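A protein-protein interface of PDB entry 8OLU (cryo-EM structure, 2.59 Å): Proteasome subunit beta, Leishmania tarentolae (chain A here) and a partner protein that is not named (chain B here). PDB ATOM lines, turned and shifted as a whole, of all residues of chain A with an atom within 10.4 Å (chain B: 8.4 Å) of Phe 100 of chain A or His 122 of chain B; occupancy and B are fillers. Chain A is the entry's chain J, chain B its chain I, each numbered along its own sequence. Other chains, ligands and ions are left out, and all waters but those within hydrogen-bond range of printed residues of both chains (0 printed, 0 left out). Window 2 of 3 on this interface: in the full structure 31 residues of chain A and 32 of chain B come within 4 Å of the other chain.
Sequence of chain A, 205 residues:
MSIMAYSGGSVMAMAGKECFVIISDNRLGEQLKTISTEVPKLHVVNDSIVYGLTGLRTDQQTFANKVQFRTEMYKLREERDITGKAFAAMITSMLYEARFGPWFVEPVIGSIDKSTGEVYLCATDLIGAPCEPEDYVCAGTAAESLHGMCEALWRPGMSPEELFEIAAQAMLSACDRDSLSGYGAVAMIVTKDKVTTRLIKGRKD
Among the printed residues, merely in contact across the chains: Phe 100 of chain A with His 122 of chain B, Arg 99 of chain A with Ser 124 of chain B, Ile 127 of chain A with Thr 77 of chain B and Arg 99 of chain A with Thr 77 of chain B.
The side-chain hydroxyl of Ser 124 of chain B is in hydrogen-bond range of the side-chain hydroxyl of Thr 77 of chain B, 2.8 Å away. N of Ser 124 of chain B is in hydrogen-bond range of OD2 of Asp 80 of chain B (3.2 Å).
Of the printed residues of chain B, Tyr 96 of chain A touches Asp 80 (2.4 Å). Of the printed residues of chain B, Arg 99 of chain A touches Thr 77 (3.96 Å), Asp 80 (2.5 Å), His 122 (3.4 Å) and Ser 124 (3.96 Å). Of the printed residues of chain B, Ile 127 of chain A touches Thr 77. Printed residues of chain A within 4 Å of Thr 77 of chain B: Arg 99 and Ile 127. Of the printed residues of chain A, Asp 80 of chain B touches Tyr 96 (2.4 Å) and Arg 99 (2.5 Å). No residue of chain A comes within 4 Å of Tyr 119 of chain B. No residue of chain A comes within 4 Å of Gly 121 of chain B. Of chain A, only Arg 99 and Phe 100 come within 4 Å of His 122 of chain B. No residue of chain A comes within 4 Å of Val 123 of chain B. Of chain A, only Arg 99 comes within 4 Å of Ser 124 of chain B. The nearest residue of chain B that does not touch Phe 100 of chain A is Val 123 of chain B (4.1 Å). The nearest residue of chain A that does not touch His 122 of chain B is Tyr 96 of chain A (6.7 Å). The nearest printed residue of chain B that does not touch Tyr 96 of chain A is Val 123 of chain B (4.2 Å).
OH of Tyr 96 of chain A is in hydrogen-bond range of OD1 of Asp 80 of chain B (2.4 Å). The guanidinium group (NH1) of Arg 99 of chain A is in salt-bridge range of the side-chain carboxylate (OD2) of Asp 80 of chain B (2.5 Å). The guanidinium group (NH1) of Arg 99 of chain A sits at hydrogen-bond distance from the backbone carbonyl oxygen (O) of His 122 of chain B.
Of the 16 printed residues of chain B, 4 touch a printed residue of chain A. Hydrophobic or aromatic side chains of chain B that line the printed part of chain A: His 122. Of the 15 printed residues of chain A, 4 touch a printed residue of chain B. Among the printed residues, 7 pairs touch across the chains. Among the printed residues, Asp or Glu carboxylates within 4 Å of a Lys or Arg side-chain nitrogen of the other chain: Arg 99 of chain A with Asp 80 of chain B.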
ATOM      1  N   SER A  93      32.967  -0.406 -26.275  1.00  0.00           N
ATOM      2  CA  SER A  93      32.214  -1.469 -26.845  1.00  0.00           C
ATOM      3  C   SER A  93      31.305  -2.140 -25.838  1.00  0.00           C
ATOM      4  O   SER A  93      30.148  -2.392 -26.115  1.00  0.00           O
ATOM      5  CB  SER A  93      33.124  -2.419 -27.416  1.00  0.00           C
ATOM      6  OG  SER A  93      32.396  -3.608 -27.576  1.00  0.00           O
ATOM      7  N   MET A  94      31.828  -2.486 -24.683  1.00  0.00           N
ATOM      8  CA  MET A  94      31.018  -3.207 -23.719  1.00  0.00           C
ATOM      9  C   MET A  94      29.854  -2.376 -23.214  1.00  0.00           C
ATOM     10  O   MET A  94      28.837  -2.890 -22.827  1.00  0.00           O
ATOM     11  CB  MET A  94      31.862  -3.598 -22.513  1.00  0.00           C
ATOM     12  CG  MET A  94      32.874  -4.633 -22.826  1.00  0.00           C
ATOM     13  SD  MET A  94      34.153  -4.732 -21.511  1.00  0.00           S
ATOM     14  CE  MET A  94      33.174  -5.639 -20.316  1.00  0.00           C
ATOM     15  N   LEU A  95      30.075  -1.115 -23.065  1.00  0.00           N
ATOM     16  CA  LEU A  95      29.040  -0.311 -22.516  1.00  0.00           C
ATOM     17  C   LEU A  95      27.936  -0.118 -23.510  1.00  0.00           C
ATOM     18  O   LEU A  95      26.806   0.041 -23.103  1.00  0.00           O
ATOM     19  CB  LEU A  95      29.639   1.031 -22.138  1.00  0.00           C
ATOM     20  CG  LEU A  95      30.476   0.985 -20.874  1.00  0.00           C
ATOM     21  CD1 LEU A  95      31.248   2.276 -20.719  1.00  0.00           C
ATOM     22  CD2 LEU A  95      29.616   0.753 -19.680  1.00  0.00           C
ATOM     23  N   TYR A  96      28.313  -0.058 -24.773  1.00  0.00           N
ATOM     24  CA  TYR A  96      27.386   0.157 -25.863  1.00  0.00           C
ATOM     25  C   TYR A  96      26.603  -1.098 -26.170  1.00  0.00           C
ATOM     26  O   TYR A  96      25.473  -0.988 -26.586  1.00  0.00           O
ATOM     27  CB  TYR A  96      28.118   0.613 -27.129  1.00  0.00           C
ATOM     28  CG  TYR A  96      27.175   1.225 -28.118  1.00  0.00           C
ATOM     29  CD1 TYR A  96      26.648   2.472 -27.876  1.00  0.00           C
ATOM     30  CD2 TYR A  96      26.734   0.535 -29.236  1.00  0.00           C
ATOM     31  CE1 TYR A  96      25.725   3.028 -28.747  1.00  0.00           C
ATOM     32  CE2 TYR A  96      25.755   1.045 -30.071  1.00  0.00           C
ATOM     33  CZ  TYR A  96      25.290   2.320 -29.851  1.00  0.00           C
ATOM     34  OH  TYR A  96      24.376   2.928 -30.679  1.00  0.00           O
ATOM     35  N   GLU A  97      27.177  -2.286 -26.034  1.00  0.00           N
ATOM     36  CA  GLU A  97      26.346  -3.470 -26.083  1.00  0.00           C
ATOM     37  C   GLU A  97      25.102  -3.264 -25.213  1.00  0.00           C
ATOM     38  O   GLU A  97      24.051  -3.863 -25.420  1.00  0.00           O
ATOM     39  CB  GLU A  97      26.961  -4.669 -25.400  1.00  0.00           C
ATOM     40  CG  GLU A  97      27.921  -5.517 -26.183  1.00  0.00           C
ATOM     41  CD  GLU A  97      28.401  -6.694 -25.306  1.00  0.00           C
ATOM     42  OE1 GLU A  97      27.516  -7.535 -24.929  1.00  0.00           O
ATOM     43  OE2 GLU A  97      29.632  -6.751 -24.917  1.00  0.00           O
ATOM     44  N   ALA A  98      25.237  -2.494 -24.152  1.00  0.00           N
ATOM     45  CA  ALA A  98      24.175  -2.450 -23.183  1.00  0.00           C
ATOM     46  C   ALA A  98      23.407  -1.153 -23.315  1.00  0.00           C
ATOM     47  O   ALA A  98      22.733  -0.706 -22.422  1.00  0.00           O
ATOM     48  CB  ALA A  98      24.782  -2.617 -21.841  1.00  0.00           C
ATOM     49  N   ARG A  99      23.477  -0.569 -24.488  1.00  0.00           N
ATOM     50  CA  ARG A  99      22.943   0.749 -24.741  1.00  0.00           C
ATOM     51  C   ARG A  99      21.490   0.880 -24.327  1.00  0.00           C
ATOM     52  O   ARG A  99      21.063   1.982 -24.017  1.00  0.00           O
ATOM     53  CB  ARG A  99      23.040   0.913 -26.250  1.00  0.00           C
ATOM     54  CG  ARG A  99      22.334   2.121 -26.841  1.00  0.00           C
ATOM     55  CD  ARG A  99      23.010   3.426 -26.614  1.00  0.00           C
ATOM     56  NE  ARG A  99      22.148   4.429 -27.255  1.00  0.00           N
ATOM     57  CZ  ARG A  99      21.264   5.176 -26.618  1.00  0.00           C
ATOM     58  NH1 ARG A  99      20.979   6.378 -27.050  1.00  0.00           N
ATOM     59  NH2 ARG A  99      20.796   4.716 -25.478  1.00  0.00           N
ATOM     60  N   PHE A 100      20.727  -0.205 -24.477  1.00  0.00           N
ATOM     61  CA  PHE A 100      19.285  -0.140 -24.295  1.00  0.00           C
ATOM     62  C   PHE A 100      18.880  -0.596 -22.899  1.00  0.00           C
ATOM     63  O   PHE A 100      17.692  -0.619 -22.577  1.00  0.00           O
ATOM     64  CB  PHE A 100      18.551  -0.816 -25.471  1.00  0.00           C
ATOM     65  CG  PHE A 100      18.603   0.107 -26.662  1.00  0.00           C
ATOM     66  CD1 PHE A 100      18.205   1.438 -26.516  1.00  0.00           C
ATOM     67  CD2 PHE A 100      19.262  -0.260 -27.824  1.00  0.00           C
ATOM     68  CE1 PHE A 100      18.399   2.355 -27.533  1.00  0.00           C
ATOM     69  CE2 PHE A 100      19.434   0.655 -28.853  1.00  0.00           C
ATOM     70  CZ  PHE A 100      18.991   1.950 -28.713  1.00  0.00           C
ATOM     71  N   GLY A 101      19.879  -0.866 -22.051  1.00  0.00           N
ATOM     72  CA  GLY A 101      19.656  -1.264 -20.669  1.00  0.00           C
ATOM     73  C   GLY A 101      20.968  -1.177 -19.931  1.00  0.00           C
ATOM     74  O   GLY A 101      21.598  -2.193 -19.669  1.00  0.00           O
ATOM     75  N   PRO A 102      21.454   0.058 -19.708  1.00  0.00           N
ATOM     76  CA  PRO A 102      22.870   0.307 -19.492  1.00  0.00           C
ATOM     77  C   PRO A 102      23.398  -0.045 -18.123  1.00  0.00           C
ATOM     78  O   PRO A 102      22.659  -0.096 -17.144  1.00  0.00           O
ATOM     79  CB  PRO A 102      23.028   1.805 -19.628  1.00  0.00           C
ATOM     80  CG  PRO A 102      21.713   2.285 -20.166  1.00  0.00           C
ATOM     81  CD  PRO A 102      20.681   1.292 -19.694  1.00  0.00           C
ATOM     82  N   TRP A 103      24.688  -0.253 -18.100  1.00  0.00           N
ATOM     83  CA  TRP A 103      25.426  -0.342 -16.894  1.00  0.00           C
ATOM     84  C   TRP A 103      25.523   1.046 -16.329  1.00  0.00           C
ATOM     85  O   TRP A 103      26.050   1.947 -16.942  1.00  0.00           O
ATOM     86  CB  TRP A 103      26.817  -0.853 -17.219  1.00  0.00           C
ATOM     87  CG  TRP A 103      26.887  -2.237 -17.759  1.00  0.00           C
ATOM     88  CD1 TRP A 103      27.326  -2.601 -18.982  1.00  0.00           C
ATOM     89  CD2 TRP A 103      26.593  -3.422 -17.054  1.00  0.00           C
ATOM     90  NE1 TRP A 103      27.198  -3.933 -19.132  1.00  0.00           N
ATOM     91  CE2 TRP A 103      26.762  -4.472 -17.953  1.00  0.00           C
ATOM     92  CE3 TRP A 103      26.145  -3.707 -15.758  1.00  0.00           C
ATOM     93  CZ2 TRP A 103      26.520  -5.811 -17.603  1.00  0.00           C
ATOM     94  CZ3 TRP A 103      25.883  -5.027 -15.411  1.00  0.00           C
ATOM     95  CH2 TRP A 103      26.073  -6.066 -16.335  1.00  0.00           C
ATOM     96  N   PHE A 104      25.105   1.217 -15.104  1.00  0.00           N
ATOM     97  CA  PHE A 104      25.185   2.513 -14.516  1.00  0.00           C
ATOM     98  C   PHE A 104      26.572   2.712 -13.982  1.00  0.00           C
ATOM     99  O   PHE A 104      26.763   2.760 -12.780  1.00  0.00           O
ATOM    100  CB  PHE A 104      24.174   2.607 -13.410  1.00  0.00           C
ATOM    101  CG  PHE A 104      22.810   2.572 -13.988  1.00  0.00           C
ATOM    102  CD1 PHE A 104      22.346   3.659 -14.702  1.00  0.00           C
ATOM    103  CD2 PHE A 104      22.035   1.434 -13.884  1.00  0.00           C
ATOM    104  CE1 PHE A 104      21.094   3.629 -15.277  1.00  0.00           C
ATOM    105  CE2 PHE A 104      20.793   1.387 -14.487  1.00  0.00           C
ATOM    106  CZ  PHE A 104      20.334   2.489 -15.183  1.00  0.00           C
ATOM    107  N   LEU A 126      27.721   6.463 -19.651  1.00  0.00           N
ATOM    108  CA  LEU A 126      27.337   5.121 -19.317  1.00  0.00           C
ATOM    109  C   LEU A 126      27.028   4.251 -20.531  1.00  0.00           C
ATOM    110  O   LEU A 126      26.945   3.041 -20.424  1.00  0.00           O
ATOM    111  CB  LEU A 126      26.154   5.213 -18.364  1.00  0.00           C
ATOM    112  CG  LEU A 126      24.767   5.432 -18.940  1.00  0.00           C
ATOM    113  CD1 LEU A 126      23.799   5.565 -17.787  1.00  0.00           C
ATOM    114  CD2 LEU A 126      24.671   6.679 -19.809  1.00  0.00           C
ATOM    115  N   ILE A 127      26.905   4.827 -21.706  1.00  0.00           N
ATOM    116  CA  ILE A 127      26.712   4.017 -22.886  1.00  0.00           C
ATOM    117  C   ILE A 127      27.951   4.070 -23.757  1.00  0.00           C
ATOM    118  O   ILE A 127      27.972   3.526 -24.846  1.00  0.00           O
ATOM    119  CB  ILE A 127      25.482   4.491 -23.653  1.00  0.00           C
ATOM    120  CG1 ILE A 127      25.572   5.985 -23.922  1.00  0.00           C
ATOM    121  CG2 ILE A 127      24.210   4.156 -22.896  1.00  0.00           C
ATOM    122  CD1 ILE A 127      24.397   6.439 -24.757  1.00  0.00           C
ATOM    123  N   GLY A 128      28.983   4.725 -23.293  1.00  0.00           N
ATOM    124  CA  GLY A 128      30.281   4.383 -23.804  1.00  0.00           C
ATOM    125  C   GLY A 128      30.813   5.371 -24.824  1.00  0.00           C
ATOM    126  O   GLY A 128      31.842   5.088 -25.439  1.00  0.00           O
ATOM    127  N   THR B  77      23.658  12.040 -29.968  1.00  0.00           N
ATOM    128  CA  THR B  77      24.168  11.325 -28.831  1.00  0.00           C
ATOM    129  C   THR B  77      25.491  10.742 -29.246  1.00  0.00           C
ATOM    130  O   THR B  77      25.484   9.756 -29.968  1.00  0.00           O
ATOM    131  CB  THR B  77      23.121  10.281 -28.423  1.00  0.00           C
ATOM    132  OG1 THR B  77      21.940  11.034 -28.105  1.00  0.00           O
ATOM    133  CG2 THR B  77      23.570   9.363 -27.295  1.00  0.00           C
ATOM    134  N   ASP B  80      26.106   7.010 -29.963  1.00  0.00           N
ATOM    135  CA  ASP B  80      25.316   6.495 -31.051  1.00  0.00           C
ATOM    136  C   ASP B  80      25.996   6.913 -32.335  1.00  0.00           C
ATOM    137  O   ASP B  80      26.201   6.126 -33.245  1.00  0.00           O
ATOM    138  CB  ASP B  80      23.887   6.986 -30.870  1.00  0.00           C
ATOM    139  CG  ASP B  80      23.069   6.154 -29.877  1.00  0.00           C
ATOM    140  OD1 ASP B  80      23.387   4.931 -29.704  1.00  0.00           O
ATOM    141  OD2 ASP B  80      22.098   6.710 -29.284  1.00  0.00           O
ATOM    142  N   HIS B 115      20.028   1.513 -40.790  1.00  0.00           N
ATOM    143  CA  HIS B 115      20.367   1.181 -39.420  1.00  0.00           C
ATOM    144  C   HIS B 115      19.549   2.095 -38.524  1.00  0.00           C
ATOM    145  O   HIS B 115      18.754   1.649 -37.725  1.00  0.00           O
ATOM    146  CB  HIS B 115      21.869   1.310 -39.175  1.00  0.00           C
ATOM    147  CG  HIS B 115      22.245   0.934 -37.778  1.00  0.00           C
ATOM    148  ND1 HIS B 115      22.272  -0.368 -37.341  1.00  0.00           N
ATOM    149  CD2 HIS B 115      22.565   1.759 -36.700  1.00  0.00           C
ATOM    150  CE1 HIS B 115      22.660  -0.343 -36.053  1.00  0.00           C
ATOM    151  NE2 HIS B 115      22.858   0.975 -35.623  1.00  0.00           N
ATOM    152  N   LEU B 116      19.664   3.390 -38.768  1.00  0.00           N
ATOM    153  CA  LEU B 116      18.945   4.303 -37.947  1.00  0.00           C
ATOM    154  C   LEU B 116      17.473   4.064 -38.044  1.00  0.00           C
ATOM    155  O   LEU B 116      16.841   4.234 -37.027  1.00  0.00           O
ATOM    156  CB  LEU B 116      19.282   5.701 -38.364  1.00  0.00           C
ATOM    157  CG  LEU B 116      20.740   6.031 -38.156  1.00  0.00           C
ATOM    158  CD1 LEU B 116      21.000   7.449 -38.604  1.00  0.00           C
ATOM    159  CD2 LEU B 116      21.139   5.913 -36.708  1.00  0.00           C
ATOM    160  N   TYR B 117      16.925   3.678 -39.187  1.00  0.00           N
ATOM    161  CA  TYR B 117      15.491   3.522 -39.312  1.00  0.00           C
ATOM    162  C   TYR B 117      15.005   2.386 -38.437  1.00  0.00           C
ATOM    163  O   TYR B 117      13.890   2.380 -37.989  1.00  0.00           O
ATOM    164  CB  TYR B 117      15.067   3.239 -40.765  1.00  0.00           C
ATOM    165  CG  TYR B 117      13.572   3.078 -40.942  1.00  0.00           C
ATOM    166  CD1 TYR B 117      12.738   4.175 -40.738  1.00  0.00           C
ATOM    167  CD2 TYR B 117      12.976   1.845 -41.148  1.00  0.00           C
ATOM    168  CE1 TYR B 117      11.360   4.065 -40.722  1.00  0.00           C
ATOM    169  CE2 TYR B 117      11.584   1.726 -41.191  1.00  0.00           C
ATOM    170  CZ  TYR B 117      10.779   2.841 -40.969  1.00  0.00           C
ATOM    171  OH  TYR B 117       9.417   2.883 -41.021  1.00  0.00           O
ATOM    172  N   ARG B 118      15.824   1.365 -38.295  1.00  0.00           N
ATOM    173  CA  ARG B 118      15.472   0.147 -37.599  1.00  0.00           C
ATOM    174  C   ARG B 118      15.380   0.403 -36.114  1.00  0.00           C
ATOM    175  O   ARG B 118      14.567  -0.183 -35.430  1.00  0.00           O
ATOM    176  CB  ARG B 118      16.577  -0.824 -37.932  1.00  0.00           C
ATOM    177  CG  ARG B 118      16.422  -2.247 -37.443  1.00  0.00           C
ATOM    178  CD  ARG B 118      17.468  -3.055 -38.234  1.00  0.00           C
ATOM    179  NE  ARG B 118      18.169  -4.023 -37.398  1.00  0.00           N
ATOM    180  CZ  ARG B 118      19.445  -3.923 -37.034  1.00  0.00           C
ATOM    181  NH1 ARG B 118      20.286  -3.157 -37.714  1.00  0.00           N
ATOM    182  NH2 ARG B 118      19.878  -4.606 -35.990  1.00  0.00           N
ATOM    183  N   TYR B 119      16.131   1.374 -35.631  1.00  0.00           N
ATOM    184  CA  TYR B 119      16.150   1.672 -34.222  1.00  0.00           C
ATOM    185  C   TYR B 119      15.179   2.788 -33.885  1.00  0.00           C
ATOM    186  O   TYR B 119      15.172   3.247 -32.744  1.00  0.00           O
ATOM    187  CB  TYR B 119      17.602   1.906 -33.802  1.00  0.00           C
ATOM    188  CG  TYR B 119      18.316   0.584 -33.680  1.00  0.00           C
ATOM    189  CD1 TYR B 119      17.934  -0.296 -32.689  1.00  0.00           C
ATOM    190  CD2 TYR B 119      19.239   0.137 -34.614  1.00  0.00           C
ATOM    191  CE1 TYR B 119      18.474  -1.563 -32.595  1.00  0.00           C
ATOM    192  CE2 TYR B 119      19.802  -1.132 -34.536  1.00  0.00           C
ATOM    193  CZ  TYR B 119      19.426  -1.985 -33.508  1.00  0.00           C
ATOM    194  OH  TYR B 119      19.933  -3.254 -33.306  1.00  0.00           O
ATOM    195  N   GLN B 120      14.405   3.241 -34.879  1.00  0.00           N
ATOM    196  CA  GLN B 120      13.283   4.152 -34.696  1.00  0.00           C
ATOM    197  C   GLN B 120      13.679   5.370 -33.873  1.00  0.00           C
ATOM    198  O   GLN B 120      12.889   5.856 -33.074  1.00  0.00           O
ATOM    199  CB  GLN B 120      12.126   3.449 -33.983  1.00  0.00           C
ATOM    200  CG  GLN B 120      11.602   2.185 -34.670  1.00  0.00           C
ATOM    201  CD  GLN B 120      10.556   2.558 -35.697  1.00  0.00           C
ATOM    202  OE1 GLN B 120       9.480   3.058 -35.341  1.00  0.00           O
ATOM    203  NE2 GLN B 120      10.876   2.350 -36.977  1.00  0.00           N
ATOM    204  N   GLY B 121      14.881   5.896 -34.094  1.00  0.00           N
ATOM    205  CA  GLY B 121      15.239   7.170 -33.507  1.00  0.00           C
ATOM    206  C   GLY B 121      15.989   7.043 -32.190  1.00  0.00           C
ATOM    207  O   GLY B 121      16.651   7.987 -31.739  1.00  0.00           O
ATOM    208  N   HIS B 122      15.943   5.830 -31.629  1.00  0.00           N
ATOM    209  CA  HIS B 122      16.519   5.528 -30.341  1.00  0.00           C
ATOM    210  C   HIS B 122      18.018   5.660 -30.395  1.00  0.00           C
ATOM    211  O   HIS B 122      18.593   6.140 -29.432  1.00  0.00           O
ATOM    212  CB  HIS B 122      16.058   4.151 -29.886  1.00  0.00           C
ATOM    213  CG  HIS B 122      14.596   4.170 -29.585  1.00  0.00           C
ATOM    214  ND1 HIS B 122      13.997   5.224 -28.932  1.00  0.00           N
ATOM    215  CD2 HIS B 122      13.618   3.294 -29.943  1.00  0.00           C
ATOM    216  CE1 HIS B 122      12.692   4.991 -28.844  1.00  0.00           C
ATOM    217  NE2 HIS B 122      12.438   3.791 -29.458  1.00  0.00           N
ATOM    218  N   VAL B 123      18.606   5.255 -31.518  1.00  0.00           N
ATOM    219  CA  VAL B 123      19.981   5.559 -31.907  1.00  0.00           C
ATOM    220  C   VAL B 123      20.009   6.969 -32.475  1.00  0.00           C
ATOM    221  O   VAL B 123      19.746   7.197 -33.638  1.00  0.00           O
ATOM    222  CB  VAL B 123      20.460   4.509 -32.917  1.00  0.00           C
ATOM    223  CG1 VAL B 123      21.842   4.807 -33.472  1.00  0.00           C
ATOM    224  CG2 VAL B 123      20.436   3.115 -32.323  1.00  0.00           C
ATOM    225  N   SER B 124      20.264   7.920 -31.603  1.00  0.00           N
ATOM    226  CA  SER B 124      20.056   9.322 -31.873  1.00  0.00           C
ATOM    227  C   SER B 124      21.323   9.907 -32.458  1.00  0.00           C
ATOM    228  O   SER B 124      21.896  10.831 -31.926  1.00  0.00           O
ATOM    229  CB  SER B 124      19.608  10.048 -30.617  1.00  0.00           C
ATOM    230  OG  SER B 124      20.145   9.406 -29.458  1.00  0.00           O
ATOM    231  N   ALA B 125      21.756   9.315 -33.562  1.00  0.00           N
ATOM    232  CA  ALA B 125      22.810   9.889 -34.368  1.00  0.00           C
ATOM    233  C   ALA B 125      22.156  10.784 -35.396  1.00  0.00           C
ATOM    234  O   ALA B 125      21.098  10.467 -35.900  1.00  0.00           O
ATOM    235  CB  ALA B 125      23.544   8.791 -35.080  1.00  0.00           C
ATOM    236  N   PRO B 144      18.113  11.060 -37.149  1.00  0.00           N
ATOM    237  CA  PRO B 144      18.055   9.868 -36.318  1.00  0.00           C
ATOM    238  C   PRO B 144      16.972   8.900 -36.717  1.00  0.00           C
ATOM    239  O   PRO B 144      17.190   7.711 -36.584  1.00  0.00           O
ATOM    240  CB  PRO B 144      17.653  10.428 -34.975  1.00  0.00           C
ATOM    241  CG  PRO B 144      18.235  11.829 -35.006  1.00  0.00           C
ATOM    242  CD  PRO B 144      17.956  12.323 -36.404  1.00  0.00           C
ATOM    243  N   HIS B 145      15.814   9.365 -37.189  1.00  0.00           N
ATOM    244  CA  HIS B 145      14.800   8.381 -37.537  1.00  0.00           C
ATOM    245  C   HIS B 145      15.127   7.724 -38.858  1.00  0.00           C
ATOM    246  O   HIS B 145      14.480   6.758 -39.213  1.00  0.00           O
ATOM    247  CB  HIS B 145      13.394   8.969 -37.529  1.00  0.00           C
ATOM    248  CG  HIS B 145      12.950   9.308 -36.158  1.00  0.00           C
ATOM    249  ND1 HIS B 145      13.356  10.467 -35.508  1.00  0.00           N
ATOM    250  CD2 HIS B 145      12.217   8.537 -35.285  1.00  0.00           C
ATOM    251  CE1 HIS B 145      12.863  10.440 -34.263  1.00  0.00           C
ATOM    252  NE2 HIS B 145      12.140   9.240 -34.107  1.00  0.00           N
ATOM    253  N   GLY B 146      16.110   8.229 -39.569  1.00  0.00           N
ATOM    254  CA  GLY B 146      16.609   7.520 -40.728  1.00  0.00           C
ATOM    255  C   GLY B 146      16.096   8.146 -42.007  1.00  0.00           C
ATOM    256  O   GLY B 146      15.985   7.480 -43.023  1.00  0.00           O
